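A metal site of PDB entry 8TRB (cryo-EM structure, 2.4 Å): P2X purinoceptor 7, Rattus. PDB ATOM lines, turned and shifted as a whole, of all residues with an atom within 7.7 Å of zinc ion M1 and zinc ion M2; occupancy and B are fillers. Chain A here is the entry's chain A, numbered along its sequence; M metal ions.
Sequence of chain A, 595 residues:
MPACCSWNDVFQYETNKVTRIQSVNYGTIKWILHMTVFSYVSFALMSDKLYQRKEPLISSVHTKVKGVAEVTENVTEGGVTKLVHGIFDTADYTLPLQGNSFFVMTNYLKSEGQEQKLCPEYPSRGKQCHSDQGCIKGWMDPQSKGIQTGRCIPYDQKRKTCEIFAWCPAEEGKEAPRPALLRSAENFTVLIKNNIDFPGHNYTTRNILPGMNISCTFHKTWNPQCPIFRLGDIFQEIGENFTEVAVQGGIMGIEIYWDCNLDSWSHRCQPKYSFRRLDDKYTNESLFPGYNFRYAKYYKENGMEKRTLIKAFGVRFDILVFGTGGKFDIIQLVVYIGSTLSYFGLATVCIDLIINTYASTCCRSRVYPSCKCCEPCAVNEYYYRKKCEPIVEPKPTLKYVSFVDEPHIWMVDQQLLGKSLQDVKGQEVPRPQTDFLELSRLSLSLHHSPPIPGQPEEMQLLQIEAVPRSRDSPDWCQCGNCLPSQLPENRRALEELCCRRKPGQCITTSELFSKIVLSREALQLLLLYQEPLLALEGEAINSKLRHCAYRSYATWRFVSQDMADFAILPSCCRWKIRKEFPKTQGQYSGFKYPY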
ATOM      1  N   VAL A 404      21.621  -2.547  27.915  1.00  0.00           N
ATOM      2  CA  VAL A 404      20.252  -2.757  28.371  1.00  0.00           C
ATOM      3  C   VAL A 404      19.921  -1.809  29.510  1.00  0.00           C
ATOM      4  O   VAL A 404      18.793  -1.301  29.620  1.00  0.00           O
ATOM      5  CB  VAL A 404      20.041  -4.229  28.760  1.00  0.00           C
ATOM      6  CG1 VAL A 404      20.798  -4.555  30.021  1.00  0.00           C
ATOM      7  CG2 VAL A 404      18.569  -4.536  28.905  1.00  0.00           C
ATOM      8  N   GLN A 422      34.101  -1.743  25.460  1.00  0.00           N
ATOM      9  CA  GLN A 422      33.269  -1.348  26.596  1.00  0.00           C
ATOM     10  C   GLN A 422      33.706  -0.010  27.172  1.00  0.00           C
ATOM     11  O   GLN A 422      32.874   0.722  27.723  1.00  0.00           O
ATOM     12  CB  GLN A 422      33.329  -2.438  27.662  1.00  0.00           C
ATOM     13  CG  GLN A 422      32.403  -2.216  28.838  1.00  0.00           C
ATOM     14  CD  GLN A 422      31.052  -2.863  28.651  1.00  0.00           C
ATOM     15  OE1 GLN A 422      30.799  -3.537  27.644  1.00  0.00           O
ATOM     16  NE2 GLN A 422      30.171  -2.654  29.602  1.00  0.00           N
ATOM     17  N   SER A 473      35.120 -13.965  35.945  1.00  0.00           N
ATOM     18  CA  SER A 473      34.490 -13.243  34.863  1.00  0.00           C
ATOM     19  C   SER A 473      35.406 -12.133  34.366  1.00  0.00           C
ATOM     20  O   SER A 473      36.253 -11.635  35.104  1.00  0.00           O
ATOM     21  CB  SER A 473      33.153 -12.652  35.330  1.00  0.00           C
ATOM     22  OG  SER A 473      32.356 -13.627  35.966  1.00  0.00           O
ATOM     23  N   PRO A 474      35.260 -11.727  33.102  1.00  0.00           N
ATOM     24  CA  PRO A 474      36.108 -10.654  32.583  1.00  0.00           C
ATOM     25  C   PRO A 474      35.935  -9.362  33.368  1.00  0.00           C
ATOM     26  O   PRO A 474      34.860  -9.070  33.890  1.00  0.00           O
ATOM     27  CB  PRO A 474      35.625 -10.495  31.133  1.00  0.00           C
ATOM     28  CG  PRO A 474      34.984 -11.778  30.802  1.00  0.00           C
ATOM     29  CD  PRO A 474      34.373 -12.275  32.066  1.00  0.00           C
ATOM     30  N   TRP A 476      35.985  -6.243  32.297  1.00  0.00           N
ATOM     31  CA  TRP A 476      35.063  -5.320  31.642  1.00  0.00           C
ATOM     32  C   TRP A 476      33.618  -5.811  31.670  1.00  0.00           C
ATOM     33  O   TRP A 476      32.713  -5.027  31.390  1.00  0.00           O
ATOM     34  CB  TRP A 476      35.488  -5.085  30.190  1.00  0.00           C
ATOM     35  CG  TRP A 476      35.863  -6.323  29.432  1.00  0.00           C
ATOM     36  CD1 TRP A 476      37.116  -6.772  29.182  1.00  0.00           C
ATOM     37  CD2 TRP A 476      34.967  -7.253  28.832  1.00  0.00           C
ATOM     38  NE1 TRP A 476      37.076  -7.934  28.455  1.00  0.00           N
ATOM     39  CE2 TRP A 476      35.754  -8.254  28.227  1.00  0.00           C
ATOM     40  CE3 TRP A 476      33.574  -7.351  28.738  1.00  0.00           C
ATOM     41  CZ2 TRP A 476      35.207  -9.336  27.548  1.00  0.00           C
ATOM     42  CZ3 TRP A 476      33.035  -8.420  28.067  1.00  0.00           C
ATOM     43  CH2 TRP A 476      33.834  -9.401  27.482  1.00  0.00           C
ATOM     44  N   CYS A 477      33.386  -7.081  32.002  1.00  0.00           N
ATOM     45  CA  CYS A 477      32.038  -7.599  32.061  1.00  0.00           C
ATOM     46  C   CYS A 477      31.314  -7.101  33.314  1.00  0.00           C
ATOM     47  O   CYS A 477      31.941  -6.749  34.317  1.00  0.00           O
ATOM     48  CB  CYS A 477      32.034  -9.116  32.035  1.00  0.00           C
ATOM     49  SG  CYS A 477      30.433  -9.855  32.397  1.00  0.00           S
ATOM     50  N   GLN A 478      29.991  -7.089  33.243  1.00  0.00           N
ATOM     51  CA  GLN A 478      29.170  -6.660  34.360  1.00  0.00           C
ATOM     52  C   GLN A 478      27.934  -7.547  34.514  1.00  0.00           C
ATOM     53  O   GLN A 478      26.940  -7.112  35.121  1.00  0.00           O
ATOM     54  CB  GLN A 478      28.718  -5.207  34.215  1.00  0.00           C
ATOM     55  CG  GLN A 478      29.738  -4.266  33.588  1.00  0.00           C
ATOM     56  CD  GLN A 478      30.724  -3.712  34.591  1.00  0.00           C
ATOM     57  OE1 GLN A 478      30.551  -3.859  35.800  1.00  0.00           O
ATOM     58  NE2 GLN A 478      31.775  -3.086  34.084  1.00  0.00           N
ATOM     59  N   CYS A 479      27.947  -8.750  33.957  1.00  0.00           N
ATOM     60  CA  CYS A 479      26.784  -9.629  34.021  1.00  0.00           C
ATOM     61  C   CYS A 479      27.111 -11.078  34.329  1.00  0.00           C
ATOM     62  O   CYS A 479      26.181 -11.859  34.554  1.00  0.00           O
ATOM     63  CB  CYS A 479      25.994  -9.563  32.707  1.00  0.00           C
ATOM     64  SG  CYS A 479      26.836 -10.239  31.256  1.00  0.00           S
ATOM     65  N   GLY A 480      28.383 -11.483  34.355  1.00  0.00           N
ATOM     66  CA  GLY A 480      28.742 -12.820  34.732  1.00  0.00           C
ATOM     67  C   GLY A 480      28.597 -13.867  33.642  1.00  0.00           C
ATOM     68  O   GLY A 480      28.708 -15.058  33.937  1.00  0.00           O
ATOM     69  N   ASN A 481      28.348 -13.452  32.398  1.00  0.00           N
ATOM     70  CA  ASN A 481      28.184 -14.373  31.285  1.00  0.00           C
ATOM     71  C   ASN A 481      29.135 -14.116  30.142  1.00  0.00           C
ATOM     72  O   ASN A 481      29.291 -14.991  29.277  1.00  0.00           O
ATOM     73  CB  ASN A 481      26.745 -14.314  30.746  1.00  0.00           C
ATOM     74  CG  ASN A 481      25.704 -14.481  31.827  1.00  0.00           C
ATOM     75  OD1 ASN A 481      25.600 -13.668  32.740  1.00  0.00           O
ATOM     76  ND2 ASN A 481      24.923 -15.545  31.733  1.00  0.00           N
ATOM     77  N   CYS A 482      29.787 -12.966  30.101  1.00  0.00           N
ATOM     78  CA  CYS A 482      30.720 -12.658  29.033  1.00  0.00           C
ATOM     79  C   CYS A 482      31.977 -13.521  29.153  1.00  0.00           C
ATOM     80  O   CYS A 482      32.485 -13.751  30.246  1.00  0.00           O
ATOM     81  CB  CYS A 482      31.099 -11.183  29.061  1.00  0.00           C
ATOM     82  SG  CYS A 482      29.730 -10.059  28.722  1.00  0.00           S
ATOM     83  N   LEU A 483      32.466 -13.995  28.013  1.00  0.00           N
ATOM     84  CA  LEU A 483      33.651 -14.817  27.954  1.00  0.00           C
ATOM     85  C   LEU A 483      34.757 -14.095  27.185  1.00  0.00           C
ATOM     86  O   LEU A 483      34.470 -13.250  26.332  1.00  0.00           O
ATOM     87  CB  LEU A 483      33.379 -16.167  27.286  1.00  0.00           C
ATOM     88  CG  LEU A 483      31.985 -16.768  27.424  1.00  0.00           C
ATOM     89  CD1 LEU A 483      31.917 -18.088  26.680  1.00  0.00           C
ATOM     90  CD2 LEU A 483      31.621 -16.954  28.873  1.00  0.00           C
ATOM     91  N   LEU A 497      32.965  -6.545  24.867  1.00  0.00           N
ATOM     92  CA  LEU A 497      31.801  -5.731  25.135  1.00  0.00           C
ATOM     93  C   LEU A 497      30.807  -6.502  25.988  1.00  0.00           C
ATOM     94  O   LEU A 497      30.546  -7.689  25.736  1.00  0.00           O
ATOM     95  CB  LEU A 497      31.143  -5.287  23.824  1.00  0.00           C
ATOM     96  CG  LEU A 497      29.928  -4.362  23.940  1.00  0.00           C
ATOM     97  CD1 LEU A 497      30.336  -2.956  24.283  1.00  0.00           C
ATOM     98  CD2 LEU A 497      29.152  -4.413  22.640  1.00  0.00           C
ATOM     99  N   CYS A 498      30.263  -5.827  26.986  1.00  0.00           N
ATOM    100  CA  CYS A 498      29.260  -6.389  27.882  1.00  0.00           C
ATOM    101  C   CYS A 498      27.885  -5.858  27.512  1.00  0.00           C
ATOM    102  O   CYS A 498      27.746  -4.770  26.937  1.00  0.00           O
ATOM    103  CB  CYS A 498      29.578  -6.044  29.338  1.00  0.00           C
ATOM    104  SG  CYS A 498      28.657  -6.985  30.566  1.00  0.00           S
ATOM    105  N   CYS A 499      26.860  -6.641  27.824  1.00  0.00           N
ATOM    106  CA  CYS A 499      25.481  -6.253  27.559  1.00  0.00           C
ATOM    107  C   CYS A 499      25.046  -5.042  28.360  1.00  0.00           C
ATOM    108  O   CYS A 499      24.013  -4.445  28.016  1.00  0.00           O
ATOM    109  CB  CYS A 499      24.555  -7.433  27.845  1.00  0.00           C
ATOM    110  SG  CYS A 499      24.453  -7.908  29.573  1.00  0.00           S
ATOM    111  N   ARG A 500      25.780  -4.659  29.398  1.00  0.00           N
ATOM    112  CA  ARG A 500      25.394  -3.530  30.232  1.00  0.00           C
ATOM    113  C   ARG A 500      26.641  -2.837  30.752  1.00  0.00           C
ATOM    114  O   ARG A 500      27.710  -3.448  30.866  1.00  0.00           O
ATOM    115  CB  ARG A 500      24.518  -3.980  31.399  1.00  0.00           C
ATOM    116  CG  ARG A 500      25.106  -5.119  32.214  1.00  0.00           C
ATOM    117  CD  ARG A 500      24.128  -5.644  33.231  1.00  0.00           C
ATOM    118  NE  ARG A 500      23.295  -4.578  33.776  1.00  0.00           N
ATOM    119  CZ  ARG A 500      21.986  -4.674  33.986  1.00  0.00           C
ATOM    120  NH1 ARG A 500      21.320  -5.788  33.705  1.00  0.00           N
ATOM    121  NH2 ARG A 500      21.328  -3.636  34.482  1.00  0.00           N
ATOM    122  N   GLY A 504      24.460  -6.092  36.872  1.00  0.00           N
ATOM    123  CA  GLY A 504      23.046  -6.392  36.852  1.00  0.00           C
ATOM    124  C   GLY A 504      22.782  -7.717  36.170  1.00  0.00           C
ATOM    125  O   GLY A 504      23.713  -8.469  35.851  1.00  0.00           O
ATOM    126  N   GLN A 505      21.499  -7.993  35.957  1.00  0.00           N
ATOM    127  CA  GLN A 505      21.107  -9.222  35.282  1.00  0.00           C
ATOM    128  C   GLN A 505      21.433  -9.141  33.797  1.00  0.00           C
ATOM    129  O   GLN A 505      21.279  -8.094  33.164  1.00  0.00           O
ATOM    130  CB  GLN A 505      19.612  -9.484  35.491  1.00  0.00           C
ATOM    131  CG  GLN A 505      18.708  -8.369  35.014  1.00  0.00           C
ATOM    132  CD  GLN A 505      17.241  -8.695  35.190  1.00  0.00           C
ATOM    133  OE1 GLN A 505      16.832  -9.855  35.084  1.00  0.00           O
ATOM    134  NE2 GLN A 505      16.439  -7.669  35.453  1.00  0.00           N
ATOM    135  N   CYS A 506      21.879 -10.259  33.246  1.00  0.00           N
ATOM    136  CA  CYS A 506      22.208 -10.307  31.833  1.00  0.00           C
ATOM    137  C   CYS A 506      20.945 -10.248  30.979  1.00  0.00           C
ATOM    138  O   CYS A 506      19.873 -10.745  31.364  1.00  0.00           O
ATOM    139  CB  CYS A 506      22.976 -11.589  31.500  1.00  0.00           C
ATOM    140  SG  CYS A 506      23.616 -11.633  29.815  1.00  0.00           S
ATOM    141  N   ILE A 507      21.070  -9.628  29.810  1.00  0.00           N
ATOM    142  CA  ILE A 507      19.972  -9.583  28.864  1.00  0.00           C
ATOM    143  C   ILE A 507      19.607 -10.974  28.383  1.00  0.00           C
ATOM    144  O   ILE A 507      18.470 -11.235  27.991  1.00  0.00           O
ATOM    145  CB  ILE A 507      20.342  -8.659  27.679  1.00  0.00           C
ATOM    146  CG1 ILE A 507      19.089  -8.260  26.900  1.00  0.00           C
ATOM    147  CG2 ILE A 507      21.328  -9.349  26.769  1.00  0.00           C
ATOM    148  CD1 ILE A 507      19.362  -7.274  25.807  1.00  0.00           C
ATOM    149  N   THR A 508      20.579 -11.899  28.395  1.00  0.00           N
ATOM    150  CA  THR A 508      20.305 -13.262  27.956  1.00  0.00           C
ATOM    151  C   THR A 508      19.240 -13.932  28.817  1.00  0.00           C
ATOM    152  O   THR A 508      18.532 -14.825  28.331  1.00  0.00           O
ATOM    153  CB  THR A 508      21.591 -14.092  27.984  1.00  0.00           C
ATOM    154  OG1 THR A 508      22.220 -13.955  29.262  1.00  0.00           O
ATOM    155  CG2 THR A 508      22.544 -13.629  26.905  1.00  0.00           C
ATOM    156  N   THR A 509      19.120 -13.529  30.073  1.00  0.00           N
ATOM    157  CA  THR A 509      18.145 -14.131  30.959  1.00  0.00           C
ATOM    158  C   THR A 509      16.715 -13.707  30.642  1.00  0.00           C
ATOM    159  O   THR A 509      15.771 -14.324  31.144  1.00  0.00           O
ATOM    160  CB  THR A 509      18.470 -13.786  32.420  1.00  0.00           C
ATOM    161  OG1 THR A 509      18.312 -12.373  32.629  1.00  0.00           O
ATOM    162  CG2 THR A 509      19.906 -14.181  32.748  1.00  0.00           C
ATOM    163  N   TYR A 553      19.108 -10.210  17.022  1.00  0.00           N
ATOM    164  CA  TYR A 553      19.486  -9.409  18.178  1.00  0.00           C
ATOM    165  C   TYR A 553      19.782  -7.971  17.779  1.00  0.00           C
ATOM    166  O   TYR A 553      19.369  -7.023  18.450  1.00  0.00           O
ATOM    167  CB  TYR A 553      20.695 -10.015  18.885  1.00  0.00           C
ATOM    168  CG  TYR A 553      21.174  -9.184  20.046  1.00  0.00           C
ATOM    169  CD1 TYR A 553      22.082  -8.151  19.850  1.00  0.00           C
ATOM    170  CD2 TYR A 553      20.728  -9.412  21.331  1.00  0.00           C
ATOM    171  CE1 TYR A 553      22.520  -7.383  20.899  1.00  0.00           C
ATOM    172  CE2 TYR A 553      21.154  -8.652  22.381  1.00  0.00           C
ATOM    173  CZ  TYR A 553      22.050  -7.637  22.165  1.00  0.00           C
ATOM    174  OH  TYR A 553      22.503  -6.867  23.207  1.00  0.00           O
ATOM    175  N   PRO A 570      27.121  -8.119  22.274  1.00  0.00           N
ATOM    176  CA  PRO A 570      27.885  -8.381  23.504  1.00  0.00           C
ATOM    177  C   PRO A 570      28.454  -9.791  23.502  1.00  0.00           C
ATOM    178  O   PRO A 570      27.936 -10.693  22.839  1.00  0.00           O
ATOM    179  CB  PRO A 570      26.851  -8.191  24.604  1.00  0.00           C
ATOM    180  CG  PRO A 570      25.741  -7.456  23.991  1.00  0.00           C
ATOM    181  CD  PRO A 570      25.712  -7.842  22.571  1.00  0.00           C
ATOM    182  N   SER A 571      29.526  -9.957  24.265  1.00  0.00           N
ATOM    183  CA  SER A 571      30.173 -11.257  24.332  1.00  0.00           C
ATOM    184  C   SER A 571      29.225 -12.323  24.887  1.00  0.00           C
ATOM    185  O   SER A 571      29.218 -13.462  24.408  1.00  0.00           O
ATOM    186  CB  SER A 571      31.436 -11.179  25.191  1.00  0.00           C
ATOM    187  OG  SER A 571      32.403 -10.335  24.595  1.00  0.00           O
ATOM    188  N   CYS A 572      28.424 -11.957  25.885  1.00  0.00           N
ATOM    189  CA  CYS A 572      27.535 -12.936  26.501  1.00  0.00           C
ATOM    190  C   CYS A 572      26.516 -13.457  25.496  1.00  0.00           C
ATOM    191  O   CYS A 572      26.368 -14.668  25.310  1.00  0.00           O
ATOM    192  CB  CYS A 572      26.831 -12.318  27.703  1.00  0.00           C
ATOM    193  SG  CYS A 572      26.428 -10.566  27.520  1.00  0.00           S
ATOM    194  N   CYS A 573      25.808 -12.543  24.827  1.00  0.00           N
ATOM    195  CA  CYS A 573      24.823 -12.939  23.828  1.00  0.00           C
ATOM    196  C   CYS A 573      25.489 -13.651  22.650  1.00  0.00           C
ATOM    197  O   CYS A 573      24.980 -14.655  22.152  1.00  0.00           O
ATOM    198  CB  CYS A 573      24.050 -11.715  23.367  1.00  0.00           C
ATOM    199  SG  CYS A 573      23.581 -10.622  24.717  1.00  0.00           S
HETATM  200 ZN    ZN M   1      25.313 -10.073  29.496  1.00  0.00          ZN
HETATM  201 ZN    ZN M   2      28.889  -9.292  30.749  1.00  0.00          ZN
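Zinc ion M2 is bound by SG of Cys 479 (2.3 Å), SG of Cys 482 (2.3 Å), SG of Cys 498 (2.3 Å) and SG of Cys 477 (2.3 Å).
N of Gln 478 touches zinc ion M2 (3.5 Å). Within 4 Å of zinc ion M2: Cys 477, Gln 478, Cys 479, Cys 482 and Cys 498.
O of Cys 506 lies within hydrogen-bond range of OG1 of Thr 509 (2.6 Å). The backbone NH of Cys 572 sits close to the side-chain sulfur of Cys 482 (3.7 Å). OD1 of Asn 481 sits close to O of Cys 479, at 2.6 Å. The side-chain hydroxyl (OG1) of Thr 508 lies close to the side-chain sulfur (SG) of Cys 506, 2.8 Å away. The side-chain sulfur of Cys 477 lies close to the backbone NH of Gly 480, 3.3 Å away. The backbone carbonyl oxygen of Trp 476 sits at hydrogen-bond distance from the side-chain amide nitrogen of Gln 478 (3.5 Å). N of Val 404 is in hydrogen-bond range of O of Cys 499 (3.1 Å). O of Gln 478 is in hydrogen-bond range of N of Gly 504 (3.2 Å).
Of the 27 residues printed, 4 come within 4 Å of zinc ion M1. The nearest printed residue that does not touch zinc ion M1 is Ile 507 (4.3 Å).
Zinc ion M1 is bound by the side-chain sulfur of Cys 572, the side-chain sulfur of Cys 506, the side-chain sulfur of Cys 499 and the side-chain sulfur of Cys 479.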
